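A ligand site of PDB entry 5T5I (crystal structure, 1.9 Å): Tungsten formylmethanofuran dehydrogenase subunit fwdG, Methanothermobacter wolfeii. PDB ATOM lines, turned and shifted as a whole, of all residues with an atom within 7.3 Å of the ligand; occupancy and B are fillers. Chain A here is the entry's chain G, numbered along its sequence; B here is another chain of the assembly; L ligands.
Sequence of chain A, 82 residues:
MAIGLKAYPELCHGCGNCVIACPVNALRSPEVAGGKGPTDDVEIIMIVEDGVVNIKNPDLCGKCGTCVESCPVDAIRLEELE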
ATOM      1  N   ALA A   7     -18.777  -6.446  18.111  1.00  0.00           N
ATOM      2  CA  ALA A   7     -17.343  -6.335  18.395  1.00  0.00           C
ATOM      3  C   ALA A   7     -17.002  -7.023  19.727  1.00  0.00           C
ATOM      4  O   ALA A   7     -17.807  -6.983  20.656  1.00  0.00           O
ATOM      5  CB  ALA A   7     -16.938  -4.871  18.459  1.00  0.00           C
ATOM      6  N   TYR A   8     -15.799  -7.610  19.803  1.00  0.00           N
ATOM      7  CA  TYR A   8     -15.204  -8.215  20.997  1.00  0.00           C
ATOM      8  C   TYR A   8     -13.889  -7.472  21.220  1.00  0.00           C
ATOM      9  O   TYR A   8     -12.811  -7.968  20.852  1.00  0.00           O
ATOM     10  CB  TYR A   8     -14.958  -9.702  20.763  1.00  0.00           C
ATOM     11  CG  TYR A   8     -16.234 -10.512  20.739  1.00  0.00           C
ATOM     12  CD1 TYR A   8     -17.044 -10.522  19.598  1.00  0.00           C
ATOM     13  CD2 TYR A   8     -16.685 -11.182  21.863  1.00  0.00           C
ATOM     14  CE1 TYR A   8     -18.248 -11.232  19.581  1.00  0.00           C
ATOM     15  CE2 TYR A   8     -17.875 -11.892  21.848  1.00  0.00           C
ATOM     16  CZ  TYR A   8     -18.663 -11.909  20.710  1.00  0.00           C
ATOM     17  OH  TYR A   8     -19.808 -12.635  20.742  1.00  0.00           O
ATOM     18  N   PRO A   9     -13.942  -6.222  21.735  1.00  0.00           N
ATOM     19  CA  PRO A   9     -12.715  -5.411  21.837  1.00  0.00           C
ATOM     20  C   PRO A   9     -11.595  -6.026  22.675  1.00  0.00           C
ATOM     21  O   PRO A   9     -10.432  -5.769  22.393  1.00  0.00           O
ATOM     22  CB  PRO A   9     -13.206  -4.084  22.427  1.00  0.00           C
ATOM     23  CG  PRO A   9     -14.501  -4.425  23.101  1.00  0.00           C
ATOM     24  CD  PRO A   9     -15.117  -5.465  22.221  1.00  0.00           C
ATOM     25  N   LEU A  11     -10.502  -9.039  22.496  1.00  0.00           N
ATOM     26  CA  LEU A  11      -9.737  -9.911  21.611  1.00  0.00           C
ATOM     27  C   LEU A  11      -9.021  -9.145  20.469  1.00  0.00           C
ATOM     28  O   LEU A  11      -8.174  -9.719  19.782  1.00  0.00           O
ATOM     29  CB  LEU A  11     -10.704 -10.920  20.964  1.00  0.00           C
ATOM     30  CG  LEU A  11     -11.541 -11.797  21.902  1.00  0.00           C
ATOM     31  CD1 LEU A  11     -12.453 -12.689  21.116  1.00  0.00           C
ATOM     32  CD2 LEU A  11     -10.652 -12.642  22.815  1.00  0.00           C
ATOM     33  N   CYS A  12      -9.386  -7.881  20.275  1.00  0.00           N
ATOM     34  CA  CYS A  12      -8.939  -7.031  19.158  1.00  0.00           C
ATOM     35  C   CYS A  12      -7.499  -6.534  19.272  1.00  0.00           C
ATOM     36  O   CYS A  12      -7.065  -6.087  20.336  1.00  0.00           O
ATOM     37  CB  CYS A  12      -9.919  -5.870  18.997  1.00  0.00           C
ATOM     38  SG  CYS A  12      -9.613  -4.827  17.559  1.00  0.00           S
ATOM     39  N   HIS A  13      -6.769  -6.543  18.138  1.00  0.00           N
ATOM     40  CA  HIS A  13      -5.388  -6.033  18.031  1.00  0.00           C
ATOM     41  C   HIS A  13      -5.372  -4.559  17.553  1.00  0.00           C
ATOM     42  O   HIS A  13      -4.320  -3.948  17.586  1.00  0.00           O
ATOM     43  CB  HIS A  13      -4.597  -6.846  16.995  1.00  0.00           C
ATOM     44  CG  HIS A  13      -4.279  -8.258  17.395  1.00  0.00           C
ATOM     45  ND1 HIS A  13      -3.186  -8.902  16.882  1.00  0.00           N
ATOM     46  CD2 HIS A  13      -4.924  -9.100  18.240  1.00  0.00           C
ATOM     47  CE1 HIS A  13      -3.200 -10.128  17.386  1.00  0.00           C
ATOM     48  NE2 HIS A  13      -4.216 -10.278  18.252  1.00  0.00           N
ATOM     49  N   GLY A  14      -6.506  -4.045  17.037  1.00  0.00           N
ATOM     50  CA  GLY A  14      -6.563  -2.705  16.476  1.00  0.00           C
ATOM     51  C   GLY A  14      -5.803  -2.632  15.167  1.00  0.00           C
ATOM     52  O   GLY A  14      -5.294  -1.569  14.811  1.00  0.00           O
ATOM     53  N   CYS A  15      -5.696  -3.768  14.452  1.00  0.00           N
ATOM     54  CA  CYS A  15      -4.924  -3.891  13.209  1.00  0.00           C
ATOM     55  C   CYS A  15      -5.532  -3.078  12.048  1.00  0.00           C
ATOM     56  O   CYS A  15      -4.799  -2.673  11.145  1.00  0.00           O
ATOM     57  CB  CYS A  15      -4.745  -5.362  12.845  1.00  0.00           C
ATOM     58  SG  CYS A  15      -6.204  -6.135  12.107  1.00  0.00           S
ATOM     59  N   GLY A  16      -6.849  -2.860  12.060  1.00  0.00           N
ATOM     60  CA  GLY A  16      -7.546  -2.099  11.034  1.00  0.00           C
ATOM     61  C   GLY A  16      -7.942  -2.855   9.774  1.00  0.00           C
ATOM     62  O   GLY A  16      -8.526  -2.245   8.886  1.00  0.00           O
ATOM     63  N   ASN A  17      -7.705  -4.184   9.695  1.00  0.00           N
ATOM     64  CA  ASN A  17      -8.077  -4.958   8.501  1.00  0.00           C
ATOM     65  C   ASN A  17      -9.566  -4.810   8.165  1.00  0.00           C
ATOM     66  O   ASN A  17      -9.908  -4.603   7.001  1.00  0.00           O
ATOM     67  CB  ASN A  17      -7.755  -6.444   8.650  1.00  0.00           C
ATOM     68  CG  ASN A  17      -6.283  -6.822   8.698  1.00  0.00           C
ATOM     69  OD1 ASN A  17      -5.388  -5.991   8.527  1.00  0.00           O
ATOM     70  ND2 ASN A  17      -6.014  -8.082   8.935  1.00  0.00           N
ATOM     71  N   CYS A  18     -10.444  -4.934   9.169  1.00  0.00           N
ATOM     72  CA  CYS A  18     -11.905  -4.842   9.010  1.00  0.00           C
ATOM     73  C   CYS A  18     -12.357  -3.471   8.514  1.00  0.00           C
ATOM     74  O   CYS A  18     -13.252  -3.390   7.667  1.00  0.00           O
ATOM     75  CB  CYS A  18     -12.626  -5.237  10.298  1.00  0.00           C
ATOM     76  SG  CYS A  18     -12.192  -4.225  11.750  1.00  0.00           S
ATOM     77  N   VAL A  19     -11.765  -2.407   9.072  1.00  0.00           N
ATOM     78  CA  VAL A  19     -12.096  -1.017   8.746  1.00  0.00           C
ATOM     79  C   VAL A  19     -11.842  -0.774   7.245  1.00  0.00           C
ATOM     80  O   VAL A  19     -12.691  -0.215   6.549  1.00  0.00           O
ATOM     81  CB  VAL A  19     -11.298  -0.022   9.648  1.00  0.00           C
ATOM     82  CG1 VAL A  19     -11.543   1.430   9.236  1.00  0.00           C
ATOM     83  CG2 VAL A  19     -11.641  -0.214  11.133  1.00  0.00           C
ATOM     84  N   MET A  46     -17.448   1.438  11.469  1.00  0.00           N
ATOM     85  CA  MET A  46     -16.558   1.244  12.611  1.00  0.00           C
ATOM     86  C   MET A  46     -15.169   1.815  12.321  1.00  0.00           C
ATOM     87  O   MET A  46     -14.782   1.964  11.162  1.00  0.00           O
ATOM     88  CB  MET A  46     -16.472  -0.256  13.040  1.00  0.00           C
ATOM     89  CG  MET A  46     -15.722  -1.180  12.062  1.00  0.00           C
ATOM     90  SD  MET A  46     -16.593  -1.459  10.486  1.00  0.00           S
ATOM     91  CE  MET A  46     -15.821  -3.007   9.957  1.00  0.00           C
ATOM     92  N   ILE A  47     -14.455   2.142  13.407  1.00  0.00           N
ATOM     93  CA  ILE A  47     -13.089   2.661  13.389  1.00  0.00           C
ATOM     94  C   ILE A  47     -12.304   2.022  14.512  1.00  0.00           C
ATOM     95  O   ILE A  47     -12.900   1.458  15.433  1.00  0.00           O
ATOM     96  CB  ILE A  47     -13.041   4.212  13.593  1.00  0.00           C
ATOM     97  CG1 ILE A  47     -13.796   4.673  14.879  1.00  0.00           C
ATOM     98  CG2 ILE A  47     -13.540   4.934  12.386  1.00  0.00           C
ATOM     99  CD1 ILE A  47     -13.537   6.118  15.260  1.00  0.00           C
ATOM    100  N   VAL A  48     -10.979   2.157  14.468  1.00  0.00           N
ATOM    101  CA  VAL A  48     -10.125   1.721  15.570  1.00  0.00           C
ATOM    102  C   VAL A  48      -9.997   2.960  16.468  1.00  0.00           C
ATOM    103  O   VAL A  48      -9.515   4.001  16.022  1.00  0.00           O
ATOM    104  CB  VAL A  48      -8.773   1.129  15.118  1.00  0.00           C
ATOM    105  CG1 VAL A  48      -7.859   0.886  16.312  1.00  0.00           C
ATOM    106  CG2 VAL A  48      -9.006  -0.176  14.356  1.00  0.00           C
ATOM    107  N   GLY A  51      -7.203   2.031  20.508  1.00  0.00           N
ATOM    108  CA  GLY A  51      -6.531   0.760  20.228  1.00  0.00           C
ATOM    109  C   GLY A  51      -7.366  -0.438  19.838  1.00  0.00           C
ATOM    110  O   GLY A  51      -6.798  -1.494  19.583  1.00  0.00           O
ATOM    111  N   VAL A  52      -8.708  -0.317  19.784  1.00  0.00           N
ATOM    112  CA  VAL A  52      -9.611  -1.420  19.475  1.00  0.00           C
ATOM    113  C   VAL A  52     -10.757  -0.992  18.555  1.00  0.00           C
ATOM    114  O   VAL A  52     -11.136   0.185  18.518  1.00  0.00           O
ATOM    115  CB  VAL A  52     -10.189  -2.056  20.767  1.00  0.00           C
ATOM    116  CG1 VAL A  52      -9.085  -2.665  21.634  1.00  0.00           C
ATOM    117  CG2 VAL A  52     -11.029  -1.052  21.571  1.00  0.00           C
ATOM    118  N   VAL A  53     -11.338  -1.977  17.872  1.00  0.00           N
ATOM    119  CA  VAL A  53     -12.491  -1.725  17.014  1.00  0.00           C
ATOM    120  C   VAL A  53     -13.669  -1.179  17.845  1.00  0.00           C
ATOM    121  O   VAL A  53     -13.917  -1.627  18.965  1.00  0.00           O
ATOM    122  CB  VAL A  53     -12.877  -2.964  16.148  1.00  0.00           C
ATOM    123  CG1 VAL A  53     -13.415  -4.126  16.997  1.00  0.00           C
ATOM    124  CG2 VAL A  53     -13.882  -2.570  15.062  1.00  0.00           C
ATOM    125  N   CYS A  67     -15.687  -8.093   6.581  1.00  0.00           N
ATOM    126  CA  CYS A  67     -14.890  -7.787   7.769  1.00  0.00           C
ATOM    127  C   CYS A  67     -14.536  -9.055   8.544  1.00  0.00           C
ATOM    128  O   CYS A  67     -13.399  -9.212   9.006  1.00  0.00           O
ATOM    129  CB  CYS A  67     -15.617  -6.792   8.666  1.00  0.00           C
ATOM    130  SG  CYS A  67     -17.272  -7.339   9.166  1.00  0.00           S
ATOM    131  N   VAL A  68     -15.506  -9.973   8.654  1.00  0.00           N
ATOM    132  CA  VAL A  68     -15.332 -11.247   9.365  1.00  0.00           C
ATOM    133  C   VAL A  68     -14.191 -12.054   8.753  1.00  0.00           C
ATOM    134  O   VAL A  68     -13.329 -12.505   9.491  1.00  0.00           O
ATOM    135  CB  VAL A  68     -16.687 -12.036   9.443  1.00  0.00           C
ATOM    136  CG1 VAL A  68     -16.505 -13.432  10.034  1.00  0.00           C
ATOM    137  CG2 VAL A  68     -17.729 -11.243  10.239  1.00  0.00           C
ATOM    138  N   SER A  70     -11.660 -10.912   7.113  1.00  0.00           N
ATOM    139  CA  SER A  70     -10.417 -10.157   7.267  1.00  0.00           C
ATOM    140  C   SER A  70      -9.816 -10.190   8.694  1.00  0.00           C
ATOM    141  O   SER A  70      -8.687  -9.734   8.883  1.00  0.00           O
ATOM    142  CB  SER A  70     -10.653  -8.703   6.834  1.00  0.00           C
ATOM    143  OG  SER A  70     -11.169  -7.904   7.884  1.00  0.00           O
ATOM    144  N   CYS A  71     -10.573 -10.706   9.697  1.00  0.00           N
ATOM    145  CA  CYS A  71     -10.096 -10.773  11.070  1.00  0.00           C
ATOM    146  C   CYS A  71      -9.622 -12.194  11.454  1.00  0.00           C
ATOM    147  O   CYS A  71     -10.451 -13.098  11.593  1.00  0.00           O
ATOM    148  CB  CYS A  71     -11.173 -10.293  12.042  1.00  0.00           C
ATOM    149  SG  CYS A  71     -10.592 -10.219  13.745  1.00  0.00           S
ATOM    150  N   PRO A  72      -8.326 -12.394  11.702  1.00  0.00           N
ATOM    151  CA  PRO A  72      -7.849 -13.745  12.073  1.00  0.00           C
ATOM    152  C   PRO A  72      -8.074 -14.139  13.542  1.00  0.00           C
ATOM    153  O   PRO A  72      -7.946 -15.327  13.878  1.00  0.00           O
ATOM    154  CB  PRO A  72      -6.353 -13.687  11.750  1.00  0.00           C
ATOM    155  CG  PRO A  72      -5.984 -12.269  11.992  1.00  0.00           C
ATOM    156  CD  PRO A  72      -7.197 -11.434  11.657  1.00  0.00           C
ATOM    157  N   VAL A  73      -8.459 -13.191  14.402  1.00  0.00           N
ATOM    158  CA  VAL A  73      -8.650 -13.418  15.844  1.00  0.00           C
ATOM    159  C   VAL A  73     -10.125 -13.384  16.285  1.00  0.00           C
ATOM    160  O   VAL A  73     -10.414 -13.415  17.481  1.00  0.00           O
ATOM    161  CB  VAL A  73      -7.764 -12.464  16.689  1.00  0.00           C
ATOM    162  CG1 VAL A  73      -6.280 -12.736  16.445  1.00  0.00           C
ATOM    163  CG2 VAL A  73      -8.092 -10.982  16.438  1.00  0.00           C
ATOM    164  N   ASP A  74     -11.062 -13.373  15.324  1.00  0.00           N
ATOM    165  CA  ASP A  74     -12.503 -13.408  15.586  1.00  0.00           C
ATOM    166  C   ASP A  74     -12.995 -12.319  16.575  1.00  0.00           C
ATOM    167  O   ASP A  74     -13.834 -12.572  17.422  1.00  0.00           O
ATOM    168  CB  ASP A  74     -12.935 -14.824  16.031  1.00  0.00           C
ATOM    169  CG  ASP A  74     -12.591 -15.917  15.031  1.00  0.00           C
ATOM    170  OD1 ASP A  74     -12.207 -15.589  13.871  1.00  0.00           O
ATOM    171  OD2 ASP A  74     -12.707 -17.104  15.409  1.00  0.00           O
ATOM    172  N   ALA A  75     -12.455 -11.108  16.410  1.00  0.00           N
ATOM    173  CA  ALA A  75     -12.792  -9.951  17.246  1.00  0.00           C
ATOM    174  C   ALA A  75     -13.958  -9.085  16.684  1.00  0.00           C
ATOM    175  O   ALA A  75     -14.428  -8.180  17.362  1.00  0.00           O
ATOM    176  CB  ALA A  75     -11.556  -9.103  17.515  1.00  0.00           C
ATOM    177  N   ILE A  76     -14.425  -9.380  15.458  1.00  0.00           N
ATOM    178  CA  ILE A  76     -15.606  -8.736  14.854  1.00  0.00           C
ATOM    179  C   ILE A  76     -16.427  -9.858  14.208  1.00  0.00           C
ATOM    180  O   ILE A  76     -15.860 -10.693  13.494  1.00  0.00           O
ATOM    181  CB  ILE A  76     -15.245  -7.558  13.906  1.00  0.00           C
ATOM    182  CG1 ILE A  76     -16.511  -6.760  13.512  1.00  0.00           C
ATOM    183  CG2 ILE A  76     -14.466  -8.024  12.674  1.00  0.00           C
ATOM    184  CD1 ILE A  76     -16.230  -5.365  13.161  1.00  0.00           C
ATOM    185  N   ARG A  77     -17.725  -9.950  14.542  1.00  0.00           N
ATOM    186  CA  ARG A  77     -18.569 -11.056  14.104  1.00  0.00           C
ATOM    187  C   ARG A  77     -19.948 -10.616  13.613  1.00  0.00           C
ATOM    188  O   ARG A  77     -20.371  -9.483  13.846  1.00  0.00           O
ATOM    189  CB  ARG A  77     -18.762 -12.039  15.295  1.00  0.00           C
ATOM    190  CG  ARG A  77     -17.438 -12.493  15.937  1.00  0.00           C
ATOM    191  CD  ARG A  77     -17.627 -13.584  16.964  1.00  0.00           C
ATOM    192  NE  ARG A  77     -16.418 -13.723  17.786  1.00  0.00           N
ATOM    193  CZ  ARG A  77     -16.323 -14.403  18.914  1.00  0.00           C
ATOM    194  NH1 ARG A  77     -17.361 -15.065  19.401  1.00  0.00           N
ATOM    195  NH2 ARG A  77     -15.171 -14.438  19.579  1.00  0.00           N
ATOM    196  N   MET B 154       0.642  -9.256  12.269  1.00  0.00           N
ATOM    197  CA  MET B 154      -0.572  -9.127  13.099  1.00  0.00           C
ATOM    198  C   MET B 154      -0.241  -8.865  14.596  1.00  0.00           C
ATOM    199  O   MET B 154      -1.013  -8.182  15.270  1.00  0.00           O
ATOM    200  CB  MET B 154      -1.445 -10.376  12.981  1.00  0.00           C
ATOM    201  CG  MET B 154      -2.279 -10.431  11.704  1.00  0.00           C
ATOM    202  SD  MET B 154      -3.488  -9.071  11.529  1.00  0.00           S
ATOM    203  CE  MET B 154      -4.259  -9.103  13.157  1.00  0.00           C
ATOM    204  N   PRO B 158       1.175  -4.162  13.708  1.00  0.00           N
ATOM    205  CA  PRO B 158      -0.252  -4.517  13.549  1.00  0.00           C
ATOM    206  C   PRO B 158      -1.021  -3.866  12.415  1.00  0.00           C
ATOM    207  O   PRO B 158      -1.878  -4.557  11.882  1.00  0.00           O
ATOM    208  CB  PRO B 158      -0.860  -4.191  14.911  1.00  0.00           C
ATOM    209  CG  PRO B 158       0.267  -4.393  15.849  1.00  0.00           C
ATOM    210  CD  PRO B 158       1.457  -3.841  15.129  1.00  0.00           C
HETATM  211 FE1  LIG L   1     -10.845  -5.491  13.049  1.00  0.00          FE
HETATM  212 FE2  LIG L   1      -8.114  -6.176  13.342  1.00  0.00          FE
HETATM  213 FE3  LIG L   1     -10.086  -8.012  13.968  1.00  0.00          FE
HETATM  214 FE4  LIG L   1      -9.725  -5.848  15.625  1.00  0.00          FE
HETATM  215  S1  LIG L   1      -8.241  -7.499  15.221  1.00  0.00           S
HETATM  216  S2  LIG L   1     -11.730  -6.635  14.786  1.00  0.00           S
HETATM  217  S3  LIG L   1      -9.172  -4.255  13.975  1.00  0.00           S
HETATM  218  S4  LIG L   1      -9.664  -7.046  11.952  1.00  0.00           S
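C of Gly 14 touches S3 of the ligand, at 3.9 Å.
CB of Asn 17 touches S4 of the ligand, at 3.9 Å.
Val 53 touches the ligand (CG1 to S2, 3.7 Å).
Val 73 touches the ligand.
CB of Ala 75 touches S2 of the ligand, at 3.7 Å.
Ile 76 touches the ligand.
Hydrophobic or aromatic side chains that line the ligand: Val 53, Val 73, Ala 75 and Ile 76.
Within 4 Å of the ligand: Cys 12, His 13, Gly 14, Cys 15, Gly 16, Asn 17, Cys 18, Val 53, Cys 71, Val 73, Ala 75 and Ile 76.
The nearest printed residue that does not touch the ligand is Val 48 (4.1 Å).
The backbone NH (N) of Ala 75 lies close to the side-chain sulfur (SG) of Cys 71 (3.4 Å).
N of Asn 17 lies close to SG of Cys 15 (3.4 Å).
N of Tyr 8 sits at hydrogen-bond distance from O of Ala 75 (2.9 Å).
The side-chain amide nitrogen of Asn 17 sits at hydrogen-bond distance from the backbone carbonyl oxygen of Ser 70.
The side-chain sulfur (SG) of Cys 12 lies close to the backbone NH (N) of Gly 14, at 3.2 Å.
The side-chain sulfur of Cys 71 sits close to the backbone NH of Val 73, at 3.7 Å.
N of Asp 74 lies close to SG of Cys 71 (3.6 Å).
The backbone NH of Val 53 lies close to the side-chain sulfur of Cys 12, at 3.3 Å.
A sulfur (S3) of the ligand lies close to the backbone NH of Cys 15 (3.5 Å).
An iron atom (FE3) of the ligand is bound by the side-chain sulfur (SG) of Cys 71.
N of His 13 lies close to S1 of the ligand, 3.4 Å away.
The backbone NH (N) of Gly 16 sits close to a sulfur (S3) of the ligand (3.3 Å).
FE1 of the ligand is bound by SG of Cys 18 (2.3 Å).
The backbone NH (N) of Cys 18 sits close to a sulfur (S4) of the ligand (3.6 Å).
An iron atom (FE4) of the ligand is bound by the side-chain sulfur (SG) of Cys 12 (2.2 Å).
An iron atom (FE2) of the ligand is bound by the side-chain sulfur of Cys 15 (2.3 Å).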
